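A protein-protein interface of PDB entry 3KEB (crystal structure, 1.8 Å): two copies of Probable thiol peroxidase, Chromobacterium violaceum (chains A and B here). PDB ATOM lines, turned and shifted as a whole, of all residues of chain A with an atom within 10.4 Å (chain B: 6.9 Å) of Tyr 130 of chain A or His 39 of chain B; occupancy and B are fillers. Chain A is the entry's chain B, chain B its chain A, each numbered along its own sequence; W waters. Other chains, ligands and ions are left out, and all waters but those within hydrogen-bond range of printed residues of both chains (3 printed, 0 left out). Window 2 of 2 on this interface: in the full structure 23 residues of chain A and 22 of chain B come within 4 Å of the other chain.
The side-chain hydroxyl (OH) of Tyr 10 of chain A sits close to the side-chain amino group (NZ) of Lys 38 of chain B.
O of Arg 115 of chain B is in hydrogen-bond range of NH1 of Arg 117 of chain A, 3.2 Å away.
The side-chain carboxylate (OD1) of Asp 35 of chain B lies within hydrogen-bond range of the backbone NH (N) of Lys 38 of chain B (3.1 Å).
N of His 39 of chain B sits at hydrogen-bond distance from OD1 of Asp 35 of chain B (3.0 Å).
The guanidinium group (NH1) of Arg 117 of chain A is in hydrogen-bond range of the side-chain hydroxyl (OG) of Ser 133 of chain A (3.0 Å).
The side-chain hydroxyl (OG) of Ser 133 of chain A lies within hydrogen-bond range of the backbone carbonyl oxygen (O) of Thr 128 of chain A, at 3.0 Å.
Among the printed residues, pairs that only touch across the chains: Tyr 130 of chain A with Lys 38 of chain B, Tyr 130 of chain A with His 39 of chain B, Pro 131 of chain A with Lys 38 of chain B, Leu 132 of chain A with Lys 38 of chain B, Ser 133 of chain A with Arg 115 of chain B, Tyr 135 of chain A with Lys 38 of chain B and Tyr 135 of chain A with Pro 93 of chain B.
Printed residues of chain B within 4 Å of Tyr 130 of chain A: Lys 38 (3.2 Å) and His 39 (3.6 Å).
Of the printed residues of chain B, Pro 131 of chain A touches Lys 38.
No residue of chain A comes within 4 Å of Asp 35 of chain B.
No residue of chain A comes within 4 Å of Gln 37 of chain B.
Of chain A, only Tyr 130 (3.6 Å) comes within 4 Å of His 39 of chain B.
Asp 40 of chain B touches none of the printed residues of chain A.
No residue of chain A comes within 4 Å of Ala 41 of chain B.
Of the printed residues of chain A, Arg 115 of chain B touches Arg 117 (3.2 Å) and Ser 133 (2.8 Å).
The nearest residue of chain B that does not touch Tyr 130 of chain A is Asp 40 of chain B (4.4 Å).
Of the 13 printed residues of chain B, 4 touch a printed residue of chain A.
Printed residues of chain A that touch a printed residue of chain B: Tyr 10, Arg 117, Tyr 130, Pro 131, Leu 132, Ser 133 and Tyr 135.
Hydrophobic or aromatic side chains of chain A within 4 Å of the printed part of chain B: Tyr 10, Tyr 130, Pro 131, Leu 132 and Tyr 135.
Among the printed residues, no Asp or Glu carboxylate lies within 4 Å of a Lys or Arg side-chain nitrogen of the other chain.
No position is printed for both chains.
Of the 9 pairs that touch across the chains among the printed residues, none has its exchanged pair printed and touching as well.
Water W2 bridges the side-chain hydroxyl (OH) of Tyr 10 of chain A (2.8 Å) and the side-chain amino group (NZ) of Lys 38 of chain B (3.3 Å).
Water W1 lies within hydrogen-bond range of the side-chain hydroxyl of Tyr 130 of chain A (2.9 Å), the backbone carbonyl oxygen of Gln 37 of chain B (2.9 Å) and a ring nitrogen (NE2) of His 39 of chain B (3.4 Å).
Water W3 bridges O of Pro 131 of chain A (3.3 Å) and O of Lys 38 of chain B (3.4 Å).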
ATOM      1  N   TRP A   7      16.585 -24.051 -27.522  1.00  0.00           N
ATOM      2  CA  TRP A   7      15.880 -24.982 -26.645  1.00  0.00           C
ATOM      3  C   TRP A   7      16.501 -26.374 -26.590  1.00  0.00           C
ATOM      4  O   TRP A   7      16.983 -26.880 -27.595  1.00  0.00           O
ATOM      5  CB  TRP A   7      14.413 -25.168 -27.123  1.00  0.00           C
ATOM      6  CG  TRP A   7      13.581 -23.881 -27.204  1.00  0.00           C
ATOM      7  CD1 TRP A   7      13.624 -22.944 -28.187  1.00  0.00           C
ATOM      8  CD2 TRP A   7      12.601 -23.447 -26.269  1.00  0.00           C
ATOM      9  NE1 TRP A   7      12.708 -21.943 -27.937  1.00  0.00           N
ATOM     10  CE2 TRP A   7      12.083 -22.225 -26.745  1.00  0.00           C
ATOM     11  CE3 TRP A   7      12.091 -23.987 -25.069  1.00  0.00           C
ATOM     12  CZ2 TRP A   7      11.080 -21.531 -26.080  1.00  0.00           C
ATOM     13  CZ3 TRP A   7      11.090 -23.294 -24.418  1.00  0.00           C
ATOM     14  CH2 TRP A   7      10.610 -22.064 -24.910  1.00  0.00           C
ATOM     15  N   VAL A   8      16.369 -27.029 -25.433  1.00  0.00           N
ATOM     16  CA  VAL A   8      16.827 -28.409 -25.260  1.00  0.00           C
ATOM     17  C   VAL A   8      15.624 -29.207 -24.822  1.00  0.00           C
ATOM     18  O   VAL A   8      14.851 -28.781 -23.934  1.00  0.00           O
ATOM     19  CB  VAL A   8      18.050 -28.558 -24.319  1.00  0.00           C
ATOM     20  CG1 VAL A   8      17.760 -28.141 -22.862  1.00  0.00           C
ATOM     21  CG2 VAL A   8      18.622 -30.072 -24.392  1.00  0.00           C
ATOM     22  N   GLN A   9      15.459 -30.337 -25.489  1.00  0.00           N
ATOM     23  CA  GLN A   9      14.427 -31.310 -25.147  1.00  0.00           C
ATOM     24  C   GLN A   9      14.984 -32.352 -24.173  1.00  0.00           C
ATOM     25  O   GLN A   9      15.962 -33.062 -24.431  1.00  0.00           O
ATOM     26  CB  GLN A   9      13.880 -31.958 -26.435  1.00  0.00           C
ATOM     27  CG  GLN A   9      12.653 -32.764 -26.261  1.00  0.00           C
ATOM     28  CD  GLN A   9      11.336 -31.975 -26.212  1.00  0.00           C
ATOM     29  OE1 GLN A   9      11.205 -30.884 -26.765  1.00  0.00           O
ATOM     30  NE2 GLN A   9      10.341 -32.567 -25.568  1.00  0.00           N
ATOM     31  N   TYR A  10      14.341 -32.421 -23.034  1.00  0.00           N
ATOM     32  CA  TYR A  10      14.639 -33.400 -21.995  1.00  0.00           C
ATOM     33  C   TYR A  10      13.415 -34.246 -21.766  1.00  0.00           C
ATOM     34  O   TYR A  10      12.474 -33.868 -21.083  1.00  0.00           O
ATOM     35  CB  TYR A  10      15.028 -32.637 -20.709  1.00  0.00           C
ATOM     36  CG  TYR A  10      15.196 -33.493 -19.480  1.00  0.00           C
ATOM     37  CD1 TYR A  10      16.154 -34.470 -19.416  1.00  0.00           C
ATOM     38  CD2 TYR A  10      14.407 -33.301 -18.387  1.00  0.00           C
ATOM     39  CE1 TYR A  10      16.357 -35.219 -18.274  1.00  0.00           C
ATOM     40  CE2 TYR A  10      14.581 -34.077 -17.236  1.00  0.00           C
ATOM     41  CZ  TYR A  10      15.529 -35.023 -17.195  1.00  0.00           C
ATOM     42  OH  TYR A  10      15.665 -35.790 -16.064  1.00  0.00           O
ATOM     43  N   GLY A  11      13.401 -35.421 -22.361  1.00  0.00           N
ATOM     44  CA  GLY A  11      12.192 -36.242 -22.400  1.00  0.00           C
ATOM     45  C   GLY A  11      11.077 -35.440 -22.994  1.00  0.00           C
ATOM     46  O   GLY A  11      11.214 -34.936 -24.100  1.00  0.00           O
ATOM     47  N   ASP A  12       9.978 -35.304 -22.267  1.00  0.00           N
ATOM     48  CA  ASP A  12       8.829 -34.581 -22.771  1.00  0.00           C
ATOM     49  C   ASP A  12       8.887 -33.081 -22.492  1.00  0.00           C
ATOM     50  O   ASP A  12       7.983 -32.363 -22.870  1.00  0.00           O
ATOM     51  CB  ASP A  12       7.511 -35.167 -22.203  1.00  0.00           C
ATOM     52  CG  ASP A  12       6.300 -34.695 -22.967  1.00  0.00           C
ATOM     53  OD1 ASP A  12       6.355 -34.701 -24.218  1.00  0.00           O
ATOM     54  OD2 ASP A  12       5.318 -34.269 -22.360  1.00  0.00           O
ATOM     55  N   GLU A  13       9.951 -32.618 -21.851  1.00  0.00           N
ATOM     56  CA  GLU A  13      10.086 -31.221 -21.478  1.00  0.00           C
ATOM     57  C   GLU A  13      10.963 -30.477 -22.518  1.00  0.00           C
ATOM     58  O   GLU A  13      11.971 -30.982 -22.957  1.00  0.00           O
ATOM     59  CB  GLU A  13      10.755 -31.119 -20.101  1.00  0.00           C
ATOM     60  CG  GLU A  13      10.110 -31.939 -18.972  1.00  0.00           C
ATOM     61  CD  GLU A  13       8.845 -31.304 -18.429  1.00  0.00           C
ATOM     62  OE1 GLU A  13       8.488 -30.202 -18.868  1.00  0.00           O
ATOM     63  OE2 GLU A  13       8.202 -31.907 -17.535  1.00  0.00           O
ATOM     64  N   MET A  14      10.595 -29.256 -22.838  1.00  0.00           N
ATOM     65  CA  MET A  14      11.331 -28.449 -23.797  1.00  0.00           C
ATOM     66  C   MET A  14      11.682 -27.144 -23.047  1.00  0.00           C
ATOM     67  O   MET A  14      10.779 -26.409 -22.645  1.00  0.00           O
ATOM     68  CB  MET A  14      10.457 -28.148 -25.005  1.00  0.00           C
ATOM     69  CG  MET A  14      11.174 -27.583 -26.141  1.00  0.00           C
ATOM     70  SD  MET A  14       9.972 -27.560 -27.740  1.00  0.00           S
ATOM     71  CE  MET A  14      11.250 -26.699 -28.895  1.00  0.00           C
ATOM     72  N   LEU A  15      12.958 -26.921 -22.851  1.00  0.00           N
ATOM     73  CA  LEU A  15      13.468 -25.885 -21.947  1.00  0.00           C
ATOM     74  C   LEU A  15      14.398 -24.917 -22.660  1.00  0.00           C
ATOM     75  O   LEU A  15      15.258 -25.313 -23.462  1.00  0.00           O
ATOM     76  CB  LEU A  15      14.236 -26.555 -20.829  1.00  0.00           C
ATOM     77  CG  LEU A  15      13.521 -27.695 -20.066  1.00  0.00           C
ATOM     78  CD1 LEU A  15      14.498 -28.367 -19.056  1.00  0.00           C
ATOM     79  CD2 LEU A  15      12.189 -27.227 -19.443  1.00  0.00           C
ATOM     80  N   PRO A  16      14.230 -23.628 -22.390  1.00  0.00           N
ATOM     81  CA  PRO A  16      15.135 -22.597 -22.878  1.00  0.00           C
ATOM     82  C   PRO A  16      16.558 -22.749 -22.371  1.00  0.00           C
ATOM     83  O   PRO A  16      16.770 -23.137 -21.217  1.00  0.00           O
ATOM     84  CB  PRO A  16      14.562 -21.317 -22.263  1.00  0.00           C
ATOM     85  CG  PRO A  16      13.247 -21.624 -21.842  1.00  0.00           C
ATOM     86  CD  PRO A  16      13.222 -23.055 -21.476  1.00  0.00           C
ATOM     87  N   ILE A  18      20.008 -20.393 -22.085  1.00  0.00           N
ATOM     88  CA  ILE A  18      20.239 -18.971 -22.034  1.00  0.00           C
ATOM     89  C   ILE A  18      21.719 -18.631 -22.079  1.00  0.00           C
ATOM     90  O   ILE A  18      22.542 -19.376 -21.536  1.00  0.00           O
ATOM     91  CB  ILE A  18      19.634 -18.396 -20.767  1.00  0.00           C
ATOM     92  CG1 ILE A  18      18.108 -18.706 -20.749  1.00  0.00           C
ATOM     93  CG2 ILE A  18      19.942 -16.921 -20.674  1.00  0.00           C
ATOM     94  CD1 ILE A  18      17.501 -18.615 -19.317  1.00  0.00           C
ATOM     95  N   ARG A 117      26.241 -19.763 -11.208  1.00  0.00           N
ATOM     96  CA  ARG A 117      25.880 -20.043 -12.622  1.00  0.00           C
ATOM     97  C   ARG A 117      26.582 -19.069 -13.557  1.00  0.00           C
ATOM     98  O   ARG A 117      26.050 -18.802 -14.693  1.00  0.00           O
ATOM     99  CB  ARG A 117      24.340 -19.918 -12.858  1.00  0.00           C
ATOM    100  CG  ARG A 117      23.394 -20.947 -12.180  1.00  0.00           C
ATOM    101  CD  ARG A 117      21.928 -20.344 -12.087  1.00  0.00           C
ATOM    102  NE  ARG A 117      20.892 -21.252 -11.529  1.00  0.00           N
ATOM    103  CZ  ARG A 117      19.566 -21.139 -11.730  1.00  0.00           C
ATOM    104  NH1 ARG A 117      18.728 -22.013 -11.175  1.00  0.00           N
ATOM    105  NH2 ARG A 117      19.060 -20.163 -12.487  1.00  0.00           N
ATOM    106  N   LEU A 126      23.102 -22.178 -19.881  1.00  0.00           N
ATOM    107  CA  LEU A 126      22.256 -22.071 -18.708  1.00  0.00           C
ATOM    108  C   LEU A 126      20.796 -22.418 -18.936  1.00  0.00           C
ATOM    109  O   LEU A 126      20.127 -21.855 -19.818  1.00  0.00           O
ATOM    110  CB  LEU A 126      22.169 -20.579 -18.295  1.00  0.00           C
ATOM    111  CG  LEU A 126      21.288 -20.260 -17.071  1.00  0.00           C
ATOM    112  CD1 LEU A 126      21.717 -20.869 -15.788  1.00  0.00           C
ATOM    113  CD2 LEU A 126      21.104 -18.757 -16.951  1.00  0.00           C
ATOM    114  N   ILE A 127      20.294 -23.275 -18.071  1.00  0.00           N
ATOM    115  CA  ILE A 127      18.859 -23.633 -18.032  1.00  0.00           C
ATOM    116  C   ILE A 127      18.326 -23.077 -16.682  1.00  0.00           C
ATOM    117  O   ILE A 127      18.929 -23.340 -15.585  1.00  0.00           O
ATOM    118  CB  ILE A 127      18.667 -25.176 -18.092  1.00  0.00           C
ATOM    119  CG1 ILE A 127      19.380 -25.842 -19.319  1.00  0.00           C
ATOM    120  CG2 ILE A 127      17.162 -25.497 -17.964  1.00  0.00           C
ATOM    121  CD1 ILE A 127      19.497 -27.399 -19.266  1.00  0.00           C
ATOM    122  N   THR A 128      17.195 -22.361 -16.704  1.00  0.00           N
ATOM    123  CA  THR A 128      16.566 -21.907 -15.472  1.00  0.00           C
ATOM    124  C   THR A 128      15.200 -22.550 -15.163  1.00  0.00           C
ATOM    125  O   THR A 128      14.635 -22.309 -14.077  1.00  0.00           O
ATOM    126  CB  THR A 128      16.396 -20.340 -15.441  1.00  0.00           C
ATOM    127  OG1 THR A 128      15.597 -19.924 -16.545  1.00  0.00           O
ATOM    128  CG2 THR A 128      17.771 -19.679 -15.563  1.00  0.00           C
ATOM    129  N   GLU A 129      14.677 -23.371 -16.076  1.00  0.00           N
ATOM    130  CA  GLU A 129      13.320 -23.832 -15.942  1.00  0.00           C
ATOM    131  C   GLU A 129      13.297 -25.277 -15.423  1.00  0.00           C
ATOM    132  O   GLU A 129      14.133 -26.084 -15.775  1.00  0.00           O
ATOM    133  CB  GLU A 129      12.666 -23.785 -17.313  1.00  0.00           C
ATOM    134  CG  GLU A 129      11.256 -23.509 -17.352  1.00  0.00           C
ATOM    135  CD  GLU A 129      10.886 -22.724 -18.630  1.00  0.00           C
ATOM    136  OE1 GLU A 129      10.407 -23.367 -19.576  1.00  0.00           O
ATOM    137  OE2 GLU A 129      11.093 -21.474 -18.666  1.00  0.00           O
ATOM    138  N   TYR A 130      12.298 -25.550 -14.588  1.00  0.00           N
ATOM    139  CA  TYR A 130      11.983 -26.875 -14.121  1.00  0.00           C
ATOM    140  C   TYR A 130      11.879 -27.816 -15.332  1.00  0.00           C
ATOM    141  O   TYR A 130      11.276 -27.432 -16.344  1.00  0.00           O
ATOM    142  CB  TYR A 130      10.630 -26.820 -13.334  1.00  0.00           C
ATOM    143  CG  TYR A 130      10.095 -28.194 -13.152  1.00  0.00           C
ATOM    144  CD1 TYR A 130       9.231 -28.764 -14.083  1.00  0.00           C
ATOM    145  CD2 TYR A 130      10.504 -28.980 -12.052  1.00  0.00           C
ATOM    146  CE1 TYR A 130       8.781 -30.094 -13.926  1.00  0.00           C
ATOM    147  CE2 TYR A 130      10.078 -30.294 -11.902  1.00  0.00           C
ATOM    148  CZ  TYR A 130       9.194 -30.849 -12.833  1.00  0.00           C
ATOM    149  OH  TYR A 130       8.775 -32.174 -12.664  1.00  0.00           O
ATOM    150  N   PRO A 131      12.431 -29.049 -15.246  1.00  0.00           N
ATOM    151  CA  PRO A 131      13.074 -29.672 -14.081  1.00  0.00           C
ATOM    152  C   PRO A 131      14.610 -29.614 -14.112  1.00  0.00           C
ATOM    153  O   PRO A 131      15.260 -30.336 -13.356  1.00  0.00           O
ATOM    154  CB  PRO A 131      12.660 -31.141 -14.224  1.00  0.00           C
ATOM    155  CG  PRO A 131      12.589 -31.381 -15.714  1.00  0.00           C
ATOM    156  CD  PRO A 131      12.094 -30.048 -16.276  1.00  0.00           C
ATOM    157  N   LEU A 132      15.178 -28.803 -14.988  1.00  0.00           N
ATOM    158  CA  LEU A 132      16.655 -28.756 -15.160  1.00  0.00           C
ATOM    159  C   LEU A 132      17.240 -27.420 -14.739  1.00  0.00           C
ATOM    160  O   LEU A 132      18.368 -27.088 -15.092  1.00  0.00           O
ATOM    161  CB  LEU A 132      17.094 -29.155 -16.557  1.00  0.00           C
ATOM    162  CG  LEU A 132      16.888 -30.571 -17.073  1.00  0.00           C
ATOM    163  CD1 LEU A 132      17.449 -30.718 -18.435  1.00  0.00           C
ATOM    164  CD2 LEU A 132      17.520 -31.665 -16.156  1.00  0.00           C
ATOM    165  N   SER A 133      16.505 -26.714 -13.910  1.00  0.00           N
ATOM    166  CA  SER A 133      16.920 -25.427 -13.385  1.00  0.00           C
ATOM    167  C   SER A 133      18.312 -25.540 -12.733  1.00  0.00           C
ATOM    168  O   SER A 133      18.529 -26.376 -11.862  1.00  0.00           O
ATOM    169  CB  SER A 133      15.910 -24.912 -12.378  1.00  0.00           C
ATOM    170  OG  SER A 133      16.325 -23.616 -11.942  1.00  0.00           O
ATOM    171  N   GLY A 134      19.254 -24.747 -13.216  1.00  0.00           N
ATOM    172  CA  GLY A 134      20.630 -24.760 -12.681  1.00  0.00           C
ATOM    173  C   GLY A 134      21.599 -25.728 -13.328  1.00  0.00           C
ATOM    174  O   GLY A 134      22.786 -25.638 -13.056  1.00  0.00           O
ATOM    175  N   TYR A 135      21.138 -26.666 -14.164  1.00  0.00           N
ATOM    176  CA  TYR A 135      22.051 -27.549 -14.877  1.00  0.00           C
ATOM    177  C   TYR A 135      22.747 -26.858 -16.024  1.00  0.00           C
ATOM    178  O   TYR A 135      22.239 -25.892 -16.560  1.00  0.00           O
ATOM    179  CB  TYR A 135      21.327 -28.735 -15.474  1.00  0.00           C
ATOM    180  CG  TYR A 135      21.040 -29.845 -14.520  1.00  0.00           C
ATOM    181  CD1 TYR A 135      21.843 -30.954 -14.476  1.00  0.00           C
ATOM    182  CD2 TYR A 135      19.954 -29.787 -13.659  1.00  0.00           C
ATOM    183  CE1 TYR A 135      21.615 -32.008 -13.610  1.00  0.00           C
ATOM    184  CE2 TYR A 135      19.706 -30.870 -12.771  1.00  0.00           C
ATOM    185  CZ  TYR A 135      20.553 -31.954 -12.774  1.00  0.00           C
ATOM    186  OH  TYR A 135      20.339 -33.002 -11.914  1.00  0.00           O
ATOM    187  N   LEU B  33      14.476 -25.256  -2.949  1.00  0.00           N
ATOM    188  CA  LEU B  33      15.503 -26.208  -3.304  1.00  0.00           C
ATOM    189  C   LEU B  33      14.953 -27.170  -4.352  1.00  0.00           C
ATOM    190  O   LEU B  33      13.821 -27.001  -4.792  1.00  0.00           O
ATOM    191  CB  LEU B  33      15.971 -26.979  -2.043  1.00  0.00           C
ATOM    192  CG  LEU B  33      16.623 -26.043  -1.010  1.00  0.00           C
ATOM    193  CD1 LEU B  33      16.925 -26.808   0.253  1.00  0.00           C
ATOM    194  CD2 LEU B  33      17.902 -25.404  -1.584  1.00  0.00           C
ATOM    195  N   VAL B  34      15.766 -28.148  -4.761  1.00  0.00           N
ATOM    196  CA  VAL B  34      15.288 -29.158  -5.684  1.00  0.00           C
ATOM    197  C   VAL B  34      15.698 -30.517  -5.164  1.00  0.00           C
ATOM    198  O   VAL B  34      16.800 -30.734  -4.714  1.00  0.00           O
ATOM    199  CB  VAL B  34      15.762 -28.897  -7.131  1.00  0.00           C
ATOM    200  CG1 VAL B  34      17.207 -28.669  -7.152  1.00  0.00           C
ATOM    201  CG2 VAL B  34      15.375 -30.050  -8.055  1.00  0.00           C
ATOM    202  N   ASP B  35      14.770 -31.444  -5.157  1.00  0.00           N
ATOM    203  CA  ASP B  35      15.036 -32.772  -4.603  1.00  0.00           C
ATOM    204  C   ASP B  35      15.647 -33.727  -5.610  1.00  0.00           C
ATOM    205  O   ASP B  35      15.860 -33.386  -6.759  1.00  0.00           O
ATOM    206  CB  ASP B  35      13.767 -33.356  -3.971  1.00  0.00           C
ATOM    207  CG  ASP B  35      12.704 -33.786  -4.972  1.00  0.00           C
ATOM    208  OD1 ASP B  35      12.935 -34.061  -6.191  1.00  0.00           O
ATOM    209  OD2 ASP B  35      11.522 -33.914  -4.480  1.00  0.00           O
ATOM    210  N   ASP B  36      15.899 -34.953  -5.178  1.00  0.00           N
ATOM    211  CA  ASP B  36      16.594 -35.898  -6.024  1.00  0.00           C
ATOM    212  C   ASP B  36      15.862 -36.371  -7.270  1.00  0.00           C
ATOM    213  O   ASP B  36      16.508 -36.886  -8.209  1.00  0.00           O
ATOM    214  CB  ASP B  36      17.139 -37.076  -5.218  1.00  0.00           C
ATOM    215  CG  ASP B  36      16.043 -37.936  -4.566  1.00  0.00           C
ATOM    216  OD1 ASP B  36      15.212 -37.412  -3.818  1.00  0.00           O
ATOM    217  OD2 ASP B  36      15.995 -39.156  -4.842  1.00  0.00           O
ATOM    218  N   GLN B  37      14.552 -36.195  -7.327  1.00  0.00           N
ATOM    219  CA  GLN B  37      13.793 -36.442  -8.560  1.00  0.00           C
ATOM    220  C   GLN B  37      13.519 -35.182  -9.341  1.00  0.00           C
ATOM    221  O   GLN B  37      12.651 -35.171 -10.200  1.00  0.00           O
ATOM    222  CB  GLN B  37      12.467 -37.105  -8.218  1.00  0.00           C
ATOM    223  CG  GLN B  37      12.669 -38.459  -7.466  1.00  0.00           C
ATOM    224  CD  GLN B  37      11.356 -39.032  -6.942  1.00  0.00           C
ATOM    225  OE1 GLN B  37      10.959 -38.765  -5.795  1.00  0.00           O
ATOM    226  NE2 GLN B  37      10.651 -39.782  -7.794  1.00  0.00           N
ATOM    227  N   LYS B  38      14.259 -34.121  -9.032  1.00  0.00           N
ATOM    228  CA  LYS B  38      14.201 -32.845  -9.779  1.00  0.00           C
ATOM    229  C   LYS B  38      12.949 -31.975  -9.537  1.00  0.00           C
ATOM    230  O   LYS B  38      12.764 -30.929 -10.197  1.00  0.00           O
ATOM    231  CB  LYS B  38      14.494 -33.051 -11.276  1.00  0.00           C
ATOM    232  CG  LYS B  38      15.824 -33.768 -11.538  1.00  0.00           C
ATOM    233  CD  LYS B  38      16.089 -33.795 -13.017  1.00  0.00           C
ATOM    234  CE  LYS B  38      17.349 -34.517 -13.478  1.00  0.00           C
ATOM    235  NZ  LYS B  38      17.333 -36.015 -13.144  1.00  0.00           N
ATOM    236  N   HIS B  39      12.190 -32.346  -8.518  1.00  0.00           N
ATOM    237  CA  HIS B  39      11.000 -31.574  -8.041  1.00  0.00           C
ATOM    238  C   HIS B  39      11.362 -30.428  -7.140  1.00  0.00           C
ATOM    239  O   HIS B  39      12.261 -30.551  -6.294  1.00  0.00           O
ATOM    240  CB  HIS B  39      10.039 -32.498  -7.301  1.00  0.00           C
ATOM    241  CG  HIS B  39       9.509 -33.591  -8.159  1.00  0.00           C
ATOM    242  ND1 HIS B  39       9.571 -34.916  -7.800  1.00  0.00           N
ATOM    243  CD2 HIS B  39       8.936 -33.555  -9.387  1.00  0.00           C
ATOM    244  CE1 HIS B  39       9.066 -35.655  -8.777  1.00  0.00           C
ATOM    245  NE2 HIS B  39       8.681 -34.851  -9.754  1.00  0.00           N
ATOM    246  N   ASP B  40      10.659 -29.313  -7.310  1.00  0.00           N
ATOM    247  CA  ASP B  40      10.801 -28.174  -6.402  1.00  0.00           C
ATOM    248  C   ASP B  40      10.504 -28.610  -4.962  1.00  0.00           C
ATOM    249  O   ASP B  40       9.628 -29.434  -4.728  1.00  0.00           O
ATOM    250  CB  ASP B  40       9.898 -27.022  -6.838  1.00  0.00           C
ATOM    251  CG  ASP B  40      10.386 -26.372  -8.115  1.00  0.00           C
ATOM    252  OD1 ASP B  40      11.568 -26.554  -8.486  1.00  0.00           O
ATOM    253  OD2 ASP B  40       9.612 -25.664  -8.763  1.00  0.00           O
ATOM    254  N   ALA B  41      11.271 -28.094  -4.008  1.00  0.00           N
ATOM    255  CA  ALA B  41      11.094 -28.445  -2.585  1.00  0.00           C
ATOM    256  C   ALA B  41      11.126 -27.136  -1.795  1.00  0.00           C
ATOM    257  O   ALA B  41      12.074 -26.359  -1.911  1.00  0.00           O
ATOM    258  CB  ALA B  41      12.207 -29.339  -2.091  1.00  0.00           C
ATOM    259  N   ALA B  42      10.074 -26.869  -1.038  1.00  0.00           N
ATOM    260  CA  ALA B  42      10.047 -25.726  -0.145  1.00  0.00           C
ATOM    261  C   ALA B  42       9.695 -26.238   1.255  1.00  0.00           C
ATOM    262  O   ALA B  42       9.396 -27.428   1.438  1.00  0.00           O
ATOM    263  CB  ALA B  42       9.001 -24.671  -0.646  1.00  0.00           C
ATOM    264  N   PRO B  93      20.975 -32.896  -8.180  1.00  0.00           N
ATOM    265  CA  PRO B  93      19.908 -33.861  -8.028  1.00  0.00           C
ATOM    266  C   PRO B  93      20.262 -35.246  -8.574  1.00  0.00           C
ATOM    267  O   PRO B  93      19.906 -36.257  -7.963  1.00  0.00           O
ATOM    268  CB  PRO B  93      18.766 -33.232  -8.793  1.00  0.00           C
ATOM    269  CG  PRO B  93      18.994 -31.753  -8.695  1.00  0.00           C
ATOM    270  CD  PRO B  93      20.514 -31.612  -8.731  1.00  0.00           C
ATOM    271  N   LEU B 111      17.942 -32.934  -0.851  1.00  0.00           N
ATOM    272  CA  LEU B 111      17.726 -31.664  -1.529  1.00  0.00           C
ATOM    273  C   LEU B 111      19.048 -31.060  -1.922  1.00  0.00           C
ATOM    274  O   LEU B 111      19.994 -31.064  -1.139  1.00  0.00           O
ATOM    275  CB  LEU B 111      16.995 -30.684  -0.614  1.00  0.00           C
ATOM    276  CG  LEU B 111      15.728 -31.238   0.068  1.00  0.00           C
ATOM    277  CD1 LEU B 111      15.029 -30.064   0.809  1.00  0.00           C
ATOM    278  CD2 LEU B 111      14.753 -31.922  -0.915  1.00  0.00           C
ATOM    279  N   ARG B 115      19.291 -25.001  -7.433  1.00  0.00           N
ATOM    280  CA  ARG B 115      18.295 -24.066  -7.991  1.00  0.00           C
ATOM    281  C   ARG B 115      18.508 -22.669  -7.398  1.00  0.00           C
ATOM    282  O   ARG B 115      18.163 -21.656  -8.026  1.00  0.00           O
ATOM    283  CB  ARG B 115      16.857 -24.610  -7.832  1.00  0.00           C
ATOM    284  CG  ARG B 115      15.721 -23.602  -7.938  1.00  0.00           C
ATOM    285  CD  ARG B 115      15.645 -22.981  -9.295  1.00  0.00           C
ATOM    286  NE  ARG B 115      15.189 -21.604  -9.181  1.00  0.00           N
ATOM    287  CZ  ARG B 115      13.921 -21.222  -9.166  1.00  0.00           C
ATOM    288  NH1 ARG B 115      12.938 -22.107  -9.289  1.00  0.00           N
ATOM    289  NH2 ARG B 115      13.637 -19.933  -9.042  1.00  0.00           N
HETATM  290  O   HOH W   1      10.869 -34.090 -12.195  1.00  0.00           O
HETATM  291  O   HOH W   2      17.086 -38.113 -15.628  1.00  0.00           O
HETATM  292  O   HOH W   3      14.223 -28.060 -11.215  1.00  0.00           O
